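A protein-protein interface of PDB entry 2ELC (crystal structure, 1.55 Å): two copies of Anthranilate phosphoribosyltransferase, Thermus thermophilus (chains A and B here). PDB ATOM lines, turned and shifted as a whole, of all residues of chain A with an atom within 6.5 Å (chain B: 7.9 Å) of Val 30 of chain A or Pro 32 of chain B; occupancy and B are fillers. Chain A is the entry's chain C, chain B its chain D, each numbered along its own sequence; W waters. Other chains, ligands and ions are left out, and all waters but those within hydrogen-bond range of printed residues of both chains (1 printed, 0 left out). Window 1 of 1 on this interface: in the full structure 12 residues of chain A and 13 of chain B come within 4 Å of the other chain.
Val 30 of chain A touches just these residues of chain B: Ser 31 (3.96 Å) and Pro 32 (3.3 Å). Ala 36 of chain A touches none of the printed residues of chain B. Of the printed residues of chain A, Pro 32 of chain B touches Gly 28 (3.2 Å) and Val 30 (3.3 Å). Of the printed residues of chain A, Pro 162 of chain B touches His 159 (3.3 Å). Of the printed residues of chain A, Val 163 of chain B touches His 159 (3.6 Å). The nearest residue of chain B that does not touch Val 30 of chain A is Val 30 of chain B (5.1 Å).
N of Glu 29 of chain A is in hydrogen-bond range of O of Ala 24 of chain A, at 3.1 Å. The backbone NH of Arg 34 of chain A lies within hydrogen-bond range of the side-chain hydroxyl of Ser 31 of chain A, 3.3 Å away. O of Leu 25 of chain B is in hydrogen-bond range of NE2 of His 159 of chain B, at 3.0 Å. A ring nitrogen (NE2) of His 159 of chain B sits at hydrogen-bond distance from the backbone NH of Gly 28 of chain B (3.5 Å). The side-chain hydroxyl of Ser 31 of chain B sits at hydrogen-bond distance from the backbone NH of Arg 34 of chain B (3.3 Å).
O of Gly 28 of chain A sits at hydrogen-bond distance from N of Val 33 of chain B (3.1 Å). N of Val 33 of chain A sits at hydrogen-bond distance from O of Gly 28 of chain B (3.0 Å). O of Gly 28 of chain A sits close to N of Pro 32 of chain B, at 3.4 Å. The backbone nitrogen (N) of Pro 32 of chain A lies close to the backbone carbonyl oxygen (O) of Gly 28 of chain B (3.4 Å).
Of the 17 printed residues of chain A, 8 touch a printed residue of chain B. Hydrophobic or aromatic side chains of chain A that line the printed part of chain B: Pro 32, Val 33 and His 159. Of the 18 printed residues of chain B, 9 touch a printed residue of chain A. Among the printed residues, no Asp or Glu carboxylate lies within 4 Å of a Lys or Arg side-chain nitrogen of the other chain.
Water W1 lies within hydrogen-bond range of O of His 159 of chain B and ND1 of His 159 of chain A.
Gly 28 of chain A touches Pro 32 of chain B, and with the chains exchanged Pro 32 of chain A touches Gly 28 of chain B. Val 30 of chain A touches Ser 31 of chain B, but with the chains exchanged Ser 31 of chain A does not touch Val 30 of chain B (4.01 Å). Val 30 of chain A touches Pro 32 of chain B, and with the chains exchanged Pro 32 of chain A touches Val 30 of chain B. Ser 31 of chain A touches its own counterpart, Ser 31 of chain B. 12 positions are printed for both chains. Of the 16 pairs that touch across the chains among the printed residues, 11 have their exchanged pair printed and touching as well.
O of Ala 27 of chain A touches CG2 of Val 33 of chain B, 3.4 Å away. Gly 28 of chain A touches Ser 31 of chain B. Glu 29 of chain A touches Ser 31 of chain B. Ser 31 of chain B touches Val 30 of chain A (CB to N, 3.96 Å). Pro 32 of chain B touches Val 30 of chain A. Ser 31 of chain A touches Gly 28 of chain B. CA of Ser 31 of chain A touches CA of Ser 31 of chain B (3.998 Å). Pro 32 of chain A touches His 159 of chain B. His 159 of chain A touches Pro 162 of chain B. CE1 of His 159 of chain A touches N of Val 163 of chain B (3.6 Å).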
ATOM      1  N   VAL A   4       2.427  16.243  15.226  1.00  0.00           N
ATOM      2  CA  VAL A   4       1.820  15.078  15.865  1.00  0.00           C
ATOM      3  C   VAL A   4       2.001  13.835  14.993  1.00  0.00           C
ATOM      4  O   VAL A   4       2.331  12.760  15.498  1.00  0.00           O
ATOM      5  CB  VAL A   4       0.315  15.309  16.146  1.00  0.00           C
ATOM      6  CG1 VAL A   4      -0.340  14.012  16.619  1.00  0.00           C
ATOM      7  CG2 VAL A   4       0.155  16.388  17.212  1.00  0.00           C
ATOM      8  N   VAL A  21       3.786  19.842  19.763  1.00  0.00           N
ATOM      9  CA  VAL A  21       3.000  18.669  20.127  1.00  0.00           C
ATOM     10  C   VAL A  21       2.373  18.847  21.506  1.00  0.00           C
ATOM     11  O   VAL A  21       1.175  18.621  21.684  1.00  0.00           O
ATOM     12  CB  VAL A  21       3.870  17.388  20.110  1.00  0.00           C
ATOM     13  CG1 VAL A  21       3.116  16.225  20.741  1.00  0.00           C
ATOM     14  CG2 VAL A  21       4.241  17.042  18.667  1.00  0.00           C
ATOM     15  N   ALA A  24      -0.283  21.667  21.592  1.00  0.00           N
ATOM     16  CA  ALA A  24      -1.544  21.188  21.032  1.00  0.00           C
ATOM     17  C   ALA A  24      -2.306  20.323  22.034  1.00  0.00           C
ATOM     18  O   ALA A  24      -3.518  20.461  22.194  1.00  0.00           O
ATOM     19  CB  ALA A  24      -1.279  20.401  19.748  1.00  0.00           C
ATOM     20  N   LEU A  25      -1.588  19.429  22.705  1.00  0.00           N
ATOM     21  CA  LEU A  25      -2.199  18.552  23.694  1.00  0.00           C
ATOM     22  C   LEU A  25      -2.813  19.378  24.821  1.00  0.00           C
ATOM     23  O   LEU A  25      -3.962  19.166  25.206  1.00  0.00           O
ATOM     24  CB  LEU A  25      -1.148  17.594  24.260  1.00  0.00           C
ATOM     25  CG  LEU A  25      -1.633  16.290  24.896  1.00  0.00           C
ATOM     26  CD1 LEU A  25      -2.553  15.552  23.933  1.00  0.00           C
ATOM     27  CD2 LEU A  25      -0.430  15.428  25.247  1.00  0.00           C
ATOM     28  N   MET A  26      -2.041  20.326  25.346  1.00  0.00           N
ATOM     29  CA  MET A  26      -2.514  21.180  26.428  1.00  0.00           C
ATOM     30  C   MET A  26      -3.653  22.096  25.995  1.00  0.00           C
ATOM     31  O   MET A  26      -4.464  22.524  26.818  1.00  0.00           O
ATOM     32  CB  MET A  26      -1.362  22.033  26.972  1.00  0.00           C
ATOM     33  CG  MET A  26      -0.289  21.248  27.722  1.00  0.00           C
ATOM     34  SD  MET A  26      -0.897  20.444  29.221  1.00  0.00           S
ATOM     35  CE  MET A  26      -1.120  18.771  28.638  1.00  0.00           C
ATOM     36  N   ALA A  27      -3.713  22.395  24.702  1.00  0.00           N
ATOM     37  CA  ALA A  27      -4.748  23.276  24.171  1.00  0.00           C
ATOM     38  C   ALA A  27      -6.036  22.537  23.824  1.00  0.00           C
ATOM     39  O   ALA A  27      -7.002  23.151  23.372  1.00  0.00           O
ATOM     40  CB  ALA A  27      -4.222  24.005  22.950  1.00  0.00           C
ATOM     41  N   GLY A  28      -6.045  21.224  24.036  1.00  0.00           N
ATOM     42  CA  GLY A  28      -7.227  20.429  23.744  1.00  0.00           C
ATOM     43  C   GLY A  28      -7.521  20.275  22.263  1.00  0.00           C
ATOM     44  O   GLY A  28      -8.679  20.095  21.874  1.00  0.00           O
ATOM     45  N   GLU A  29      -6.478  20.320  21.440  1.00  0.00           N
ATOM     46  CA  GLU A  29      -6.611  20.207  19.989  1.00  0.00           C
ATOM     47  C   GLU A  29      -6.316  18.816  19.450  1.00  0.00           C
ATOM     48  O   GLU A  29      -6.441  18.575  18.248  1.00  0.00           O
ATOM     49  CB  GLU A  29      -5.661  21.187  19.303  1.00  0.00           C
ATOM     50  CG  GLU A  29      -5.984  22.650  19.512  1.00  0.00           C
ATOM     51  CD  GLU A  29      -4.810  23.541  19.168  1.00  0.00           C
ATOM     52  OE1 GLU A  29      -3.953  23.112  18.369  1.00  0.00           O
ATOM     53  OE2 GLU A  29      -4.751  24.676  19.685  1.00  0.00           O
ATOM     54  N   VAL A  30      -5.921  17.902  20.328  1.00  0.00           N
ATOM     55  CA  VAL A  30      -5.575  16.556  19.890  1.00  0.00           C
ATOM     56  C   VAL A  30      -6.620  15.519  20.287  1.00  0.00           C
ATOM     57  O   VAL A  30      -7.030  15.436  21.444  1.00  0.00           O
ATOM     58  CB  VAL A  30      -4.198  16.135  20.459  1.00  0.00           C
ATOM     59  CG1 VAL A  30      -3.794  14.778  19.912  1.00  0.00           C
ATOM     60  CG2 VAL A  30      -3.143  17.177  20.095  1.00  0.00           C
ATOM     61  N   SER A  31      -7.051  14.723  19.313  1.00  0.00           N
ATOM     62  CA  SER A  31      -8.041  13.688  19.574  1.00  0.00           C
ATOM     63  C   SER A  31      -7.452  12.610  20.480  1.00  0.00           C
ATOM     64  O   SER A  31      -6.235  12.413  20.519  1.00  0.00           O
ATOM     65  CB  SER A  31      -8.497  13.046  18.262  1.00  0.00           C
ATOM     66  OG  SER A  31      -7.441  12.315  17.670  1.00  0.00           O
ATOM     67  N   PRO A  32      -8.309  11.903  21.229  1.00  0.00           N
ATOM     68  CA  PRO A  32      -7.830  10.843  22.121  1.00  0.00           C
ATOM     69  C   PRO A  32      -6.984   9.801  21.380  1.00  0.00           C
ATOM     70  O   PRO A  32      -5.980   9.314  21.897  1.00  0.00           O
ATOM     71  CB  PRO A  32      -9.124  10.254  22.673  1.00  0.00           C
ATOM     72  CG  PRO A  32     -10.020  11.460  22.748  1.00  0.00           C
ATOM     73  CD  PRO A  32      -9.749  12.155  21.433  1.00  0.00           C
ATOM     74  N   VAL A  33      -7.399   9.449  20.166  1.00  0.00           N
ATOM     75  CA  VAL A  33      -6.663   8.467  19.377  1.00  0.00           C
ATOM     76  C   VAL A  33      -5.256   8.943  19.017  1.00  0.00           C
ATOM     77  O   VAL A  33      -4.284   8.198  19.162  1.00  0.00           O
ATOM     78  CB  VAL A  33      -7.445   8.101  18.087  1.00  0.00           C
ATOM     79  CG1 VAL A  33      -6.525   7.418  17.074  1.00  0.00           C
ATOM     80  CG2 VAL A  33      -8.596   7.169  18.440  1.00  0.00           C
ATOM     81  N   ARG A  34      -5.131  10.183  18.555  1.00  0.00           N
ATOM     82  CA  ARG A  34      -3.812  10.679  18.195  1.00  0.00           C
ATOM     83  C   ARG A  34      -2.963  10.936  19.436  1.00  0.00           C
ATOM     84  O   ARG A  34      -1.743  10.802  19.392  1.00  0.00           O
ATOM     85  CB  ARG A  34      -3.931  11.938  17.332  1.00  0.00           C
ATOM     86  CG  ARG A  34      -4.686  11.690  16.027  1.00  0.00           C
ATOM     87  CD  ARG A  34      -4.619  12.902  15.121  1.00  0.00           C
ATOM     88  NE  ARG A  34      -3.341  12.971  14.422  1.00  0.00           N
ATOM     89  CZ  ARG A  34      -2.779  14.097  13.994  1.00  0.00           C
ATOM     90  NH1 ARG A  34      -3.375  15.264  14.199  1.00  0.00           N
ATOM     91  NH2 ARG A  34      -1.626  14.051  13.346  1.00  0.00           N
ATOM     92  N   ALA A  35      -3.603  11.288  20.547  1.00  0.00           N
ATOM     93  CA  ALA A  35      -2.857  11.512  21.784  1.00  0.00           C
ATOM     94  C   ALA A  35      -2.274  10.175  22.237  1.00  0.00           C
ATOM     95  O   ALA A  35      -1.107  10.088  22.618  1.00  0.00           O
ATOM     96  CB  ALA A  35      -3.769  12.074  22.861  1.00  0.00           C
ATOM     97  N   ALA A  36      -3.088   9.124  22.176  1.00  0.00           N
ATOM     98  CA  ALA A  36      -2.641   7.792  22.567  1.00  0.00           C
ATOM     99  C   ALA A  36      -1.487   7.359  21.672  1.00  0.00           C
ATOM    100  O   ALA A  36      -0.467   6.847  22.146  1.00  0.00           O
ATOM    101  CB  ALA A  36      -3.792   6.797  22.445  1.00  0.00           C
ATOM    102  N   LEU A  38       0.657   9.233  19.840  1.00  0.00           N
ATOM    103  CA  LEU A  38       1.895   9.979  20.013  1.00  0.00           C
ATOM    104  C   LEU A  38       2.591   9.619  21.321  1.00  0.00           C
ATOM    105  O   LEU A  38       3.817   9.501  21.360  1.00  0.00           O
ATOM    106  CB  LEU A  38       1.627  11.484  19.912  1.00  0.00           C
ATOM    107  CG  LEU A  38       0.998  12.247  21.074  1.00  0.00           C
ATOM    108  CD1 LEU A  38       2.097  12.647  22.055  1.00  0.00           C
ATOM    109  CD2 LEU A  38       0.296  13.494  20.552  1.00  0.00           C
ATOM    110  N   HIS A 159      -8.054  15.588  30.435  1.00  0.00           N
ATOM    111  CA  HIS A 159      -8.289  14.686  29.299  1.00  0.00           C
ATOM    112  C   HIS A 159      -7.129  13.700  29.052  1.00  0.00           C
ATOM    113  O   HIS A 159      -7.276  12.680  28.392  1.00  0.00           O
ATOM    114  CB  HIS A 159      -8.521  15.541  28.053  1.00  0.00           C
ATOM    115  CG  HIS A 159      -9.550  16.599  28.356  1.00  0.00           C
ATOM    116  ND1 HIS A 159     -10.885  16.361  28.352  1.00  0.00           N
ATOM    117  CD2 HIS A 159      -9.340  17.937  28.701  1.00  0.00           C
ATOM    118  CE1 HIS A 159     -11.463  17.528  28.691  1.00  0.00           C
ATOM    119  NE2 HIS A 159     -10.562  18.491  28.906  1.00  0.00           N
ATOM    120  N   LEU B  25     -17.112  10.663  18.103  1.00  0.00           N
ATOM    121  CA  LEU B  25     -16.843  11.049  19.478  1.00  0.00           C
ATOM    122  C   LEU B  25     -16.412   9.844  20.308  1.00  0.00           C
ATOM    123  O   LEU B  25     -15.400   9.861  20.997  1.00  0.00           O
ATOM    124  CB  LEU B  25     -18.119  11.656  20.062  1.00  0.00           C
ATOM    125  CG  LEU B  25     -17.885  12.312  21.425  1.00  0.00           C
ATOM    126  CD1 LEU B  25     -16.702  13.282  21.410  1.00  0.00           C
ATOM    127  CD2 LEU B  25     -19.091  13.115  21.913  1.00  0.00           C
ATOM    128  N   GLY B  28     -12.972   8.284  19.618  1.00  0.00           N
ATOM    129  CA  GLY B  28     -11.789   9.058  19.966  1.00  0.00           C
ATOM    130  C   GLY B  28     -11.214   9.883  18.832  1.00  0.00           C
ATOM    131  O   GLY B  28     -10.013  10.169  18.811  1.00  0.00           O
ATOM    132  N   GLU B  29     -12.069  10.277  17.893  1.00  0.00           N
ATOM    133  CA  GLU B  29     -11.656  11.070  16.736  1.00  0.00           C
ATOM    134  C   GLU B  29     -11.868  12.565  16.917  1.00  0.00           C
ATOM    135  O   GLU B  29     -11.470  13.356  16.061  1.00  0.00           O
ATOM    136  CB  GLU B  29     -12.443  10.651  15.490  1.00  0.00           C
ATOM    137  CG  GLU B  29     -12.179   9.255  14.980  1.00  0.00           C
ATOM    138  CD  GLU B  29     -12.992   8.952  13.735  1.00  0.00           C
ATOM    139  OE1 GLU B  29     -14.214   8.728  13.859  1.00  0.00           O
ATOM    140  OE2 GLU B  29     -12.411   8.952  12.626  1.00  0.00           O
ATOM    141  N   VAL B  30     -12.499  12.956  18.016  1.00  0.00           N
ATOM    142  CA  VAL B  30     -12.800  14.363  18.244  1.00  0.00           C
ATOM    143  C   VAL B  30     -11.995  14.967  19.387  1.00  0.00           C
ATOM    144  O   VAL B  30     -11.969  14.427  20.491  1.00  0.00           O
ATOM    145  CB  VAL B  30     -14.311  14.537  18.529  1.00  0.00           C
ATOM    146  CG1 VAL B  30     -14.676  16.012  18.619  1.00  0.00           C
ATOM    147  CG2 VAL B  30     -15.120  13.856  17.425  1.00  0.00           C
ATOM    148  N   SER B  31     -11.331  16.085  19.108  1.00  0.00           N
ATOM    149  CA  SER B  31     -10.528  16.771  20.113  1.00  0.00           C
ATOM    150  C   SER B  31     -11.435  17.284  21.228  1.00  0.00           C
ATOM    151  O   SER B  31     -12.638  17.468  21.035  1.00  0.00           O
ATOM    152  CB  SER B  31      -9.791  17.953  19.481  1.00  0.00           C
ATOM    153  OG  SER B  31     -10.711  18.966  19.107  1.00  0.00           O
ATOM    154  N   PRO B  32     -10.870  17.519  22.422  1.00  0.00           N
ATOM    155  CA  PRO B  32     -11.674  18.017  23.540  1.00  0.00           C
ATOM    156  C   PRO B  32     -12.410  19.319  23.207  1.00  0.00           C
ATOM    157  O   PRO B  32     -13.571  19.486  23.569  1.00  0.00           O
ATOM    158  CB  PRO B  32     -10.640  18.193  24.652  1.00  0.00           C
ATOM    159  CG  PRO B  32      -9.704  17.071  24.385  1.00  0.00           C
ATOM    160  CD  PRO B  32      -9.525  17.128  22.879  1.00  0.00           C
ATOM    161  N   VAL B  33     -11.732  20.232  22.513  1.00  0.00           N
ATOM    162  CA  VAL B  33     -12.330  21.512  22.139  1.00  0.00           C
ATOM    163  C   VAL B  33     -13.538  21.350  21.217  1.00  0.00           C
ATOM    164  O   VAL B  33     -14.578  21.953  21.450  1.00  0.00           O
ATOM    165  CB  VAL B  33     -11.280  22.442  21.475  1.00  0.00           C
ATOM    166  CG1 VAL B  33     -11.966  23.608  20.762  1.00  0.00           C
ATOM    167  CG2 VAL B  33     -10.340  22.980  22.542  1.00  0.00           C
ATOM    168  N   ARG B  34     -13.408  20.536  20.176  1.00  0.00           N
ATOM    169  CA  ARG B  34     -14.525  20.339  19.263  1.00  0.00           C
ATOM    170  C   ARG B  34     -15.642  19.537  19.922  1.00  0.00           C
ATOM    171  O   ARG B  34     -16.816  19.743  19.628  1.00  0.00           O
ATOM    172  CB  ARG B  34     -14.032  19.682  17.971  1.00  0.00           C
ATOM    173  CG  ARG B  34     -13.094  20.585  17.177  1.00  0.00           C
ATOM    174  CD  ARG B  34     -12.517  19.885  15.958  1.00  0.00           C
ATOM    175  NE  ARG B  34     -13.530  19.583  14.951  1.00  0.00           N
ATOM    176  CZ  ARG B  34     -14.155  20.498  14.217  1.00  0.00           C
ATOM    177  NH1 ARG B  34     -13.874  21.785  14.373  1.00  0.00           N
ATOM    178  NH2 ARG B  34     -15.055  20.124  13.315  1.00  0.00           N
ATOM    179  N   ALA B  35     -15.275  18.639  20.830  1.00  0.00           N
ATOM    180  CA  ALA B  35     -16.269  17.848  21.548  1.00  0.00           C
ATOM    181  C   ALA B  35     -17.096  18.772  22.443  1.00  0.00           C
ATOM    182  O   ALA B  35     -18.321  18.652  22.525  1.00  0.00           O
ATOM    183  CB  ALA B  35     -15.580  16.775  22.394  1.00  0.00           C
ATOM    184  N   ALA B  36     -16.421  19.699  23.113  1.00  0.00           N
ATOM    185  CA  ALA B  36     -17.098  20.643  23.987  1.00  0.00           C
ATOM    186  C   ALA B  36     -18.038  21.533  23.182  1.00  0.00           C
ATOM    187  O   ALA B  36     -19.172  21.782  23.590  1.00  0.00           O
ATOM    188  CB  ALA B  36     -16.070  21.500  24.725  1.00  0.00           C
ATOM    189  N   GLY B  37     -17.553  22.015  22.045  1.00  0.00           N
ATOM    190  CA  GLY B  37     -18.360  22.879  21.203  1.00  0.00           C
ATOM    191  C   GLY B  37     -19.598  22.182  20.687  1.00  0.00           C
ATOM    192  O   GLY B  37     -20.688  22.750  20.692  1.00  0.00           O
ATOM    193  N   LEU B  38     -19.428  20.943  20.244  1.00  0.00           N
ATOM    194  CA  LEU B  38     -20.534  20.163  19.711  1.00  0.00           C
ATOM    195  C   LEU B  38     -21.592  19.880  20.776  1.00  0.00           C
ATOM    196  O   LEU B  38     -22.785  20.030  20.525  1.00  0.00           O
ATOM    197  CB  LEU B  38     -19.991  18.861  19.109  1.00  0.00           C
ATOM    198  CG  LEU B  38     -19.667  17.633  19.957  1.00  0.00           C
ATOM    199  CD1 LEU B  38     -20.944  16.859  20.260  1.00  0.00           C
ATOM    200  CD2 LEU B  38     -18.705  16.745  19.183  1.00  0.00           C
ATOM    201  N   LEU B  39     -21.159  19.490  21.971  1.00  0.00           N
ATOM    202  CA  LEU B  39     -22.104  19.190  23.039  1.00  0.00           C
ATOM    203  C   LEU B  39     -22.901  20.415  23.478  1.00  0.00           C
ATOM    204  O   LEU B  39     -24.105  20.330  23.735  1.00  0.00           O
ATOM    205  CB  LEU B  39     -21.375  18.562  24.238  1.00  0.00           C
ATOM    206  CG  LEU B  39     -20.807  17.158  23.981  1.00  0.00           C
ATOM    207  CD1 LEU B  39     -20.041  16.685  25.203  1.00  0.00           C
ATOM    208  CD2 LEU B  39     -21.936  16.180  23.650  1.00  0.00           C
ATOM    209  N   HIS B 159     -12.650   8.724  27.667  1.00  0.00           N
ATOM    210  CA  HIS B 159     -12.067   9.939  27.105  1.00  0.00           C
ATOM    211  C   HIS B 159     -13.092  11.043  26.873  1.00  0.00           C
ATOM    212  O   HIS B 159     -12.727  12.177  26.553  1.00  0.00           O
ATOM    213  CB  HIS B 159     -11.304   9.637  25.802  1.00  0.00           C
ATOM    214  CG  HIS B 159     -12.157   9.104  24.693  1.00  0.00           C
ATOM    215  ND1 HIS B 159     -12.186   7.766  24.351  1.00  0.00           N
ATOM    216  CD2 HIS B 159     -13.008   9.724  23.843  1.00  0.00           C
ATOM    217  CE1 HIS B 159     -13.017   7.590  23.342  1.00  0.00           C
ATOM    218  NE2 HIS B 159     -13.532   8.762  23.012  1.00  0.00           N
ATOM    219  N   PRO B 162     -14.248  13.447  30.790  1.00  0.00           N
ATOM    220  CA  PRO B 162     -13.565  14.687  31.192  1.00  0.00           C
ATOM    221  C   PRO B 162     -14.190  15.947  30.584  1.00  0.00           C
ATOM    222  O   PRO B 162     -14.309  16.981  31.246  1.00  0.00           O
ATOM    223  CB  PRO B 162     -12.137  14.467  30.704  1.00  0.00           C
ATOM    224  CG  PRO B 162     -11.974  12.983  30.803  1.00  0.00           C
ATOM    225  CD  PRO B 162     -13.281  12.472  30.254  1.00  0.00           C
ATOM    226  N   VAL B 163     -14.579  15.861  29.317  1.00  0.00           N
ATOM    227  CA  VAL B 163     -15.195  16.998  28.641  1.00  0.00           C
ATOM    228  C   VAL B 163     -16.520  17.334  29.314  1.00  0.00           C
ATOM    229  O   VAL B 163     -16.831  18.499  29.564  1.00  0.00           O
ATOM    230  CB  VAL B 163     -15.443  16.687  27.150  1.00  0.00           C
ATOM    231  CG1 VAL B 163     -16.156  17.855  26.480  1.00  0.00           C
ATOM    232  CG2 VAL B 163     -14.123  16.410  26.458  1.00  0.00           C
ATOM    233  N   ARG B 164     -17.298  16.303  29.617  1.00  0.00           N
ATOM    234  CA  ARG B 164     -18.587  16.490  30.267  1.00  0.00           C
ATOM    235  C   ARG B 164     -18.422  17.130  31.642  1.00  0.00           C
ATOM    236  O   ARG B 164     -19.140  18.065  31.997  1.00  0.00           O
ATOM    237  CB  ARG B 164     -19.291  15.142  30.422  1.00  0.00           C
ATOM    238  CG  ARG B 164     -19.528  14.417  29.107  1.00  0.00           C
ATOM    239  CD  ARG B 164     -20.041  13.013  29.355  1.00  0.00           C
ATOM    240  NE  ARG B 164     -21.276  13.024  30.134  1.00  0.00           N
ATOM    241  CZ  ARG B 164     -21.874  11.933  30.603  1.00  0.00           C
ATOM    242  NH1 ARG B 164     -21.350  10.736  30.376  1.00  0.00           N
ATOM    243  NH2 ARG B 164     -23.002  12.037  31.289  1.00  0.00           N
ATOM    244  N   LEU B 167     -17.353  20.852  31.365  1.00  0.00           N
ATOM    245  CA  LEU B 167     -18.444  21.728  30.952  1.00  0.00           C
ATOM    246  C   LEU B 167     -19.361  22.000  32.138  1.00  0.00           C
ATOM    247  O   LEU B 167     -19.921  23.083  32.264  1.00  0.00           O
ATOM    248  CB  LEU B 167     -19.240  21.105  29.800  1.00  0.00           C
ATOM    249  CG  LEU B 167     -18.567  21.123  28.426  1.00  0.00           C
ATOM    250  CD1 LEU B 167     -19.449  20.381  27.433  1.00  0.00           C
ATOM    251  CD2 LEU B 167     -18.341  22.562  27.963  1.00  0.00           C
HETATM  252  O   HOH W   1     -10.967  13.919  26.318  1.00  0.00           O
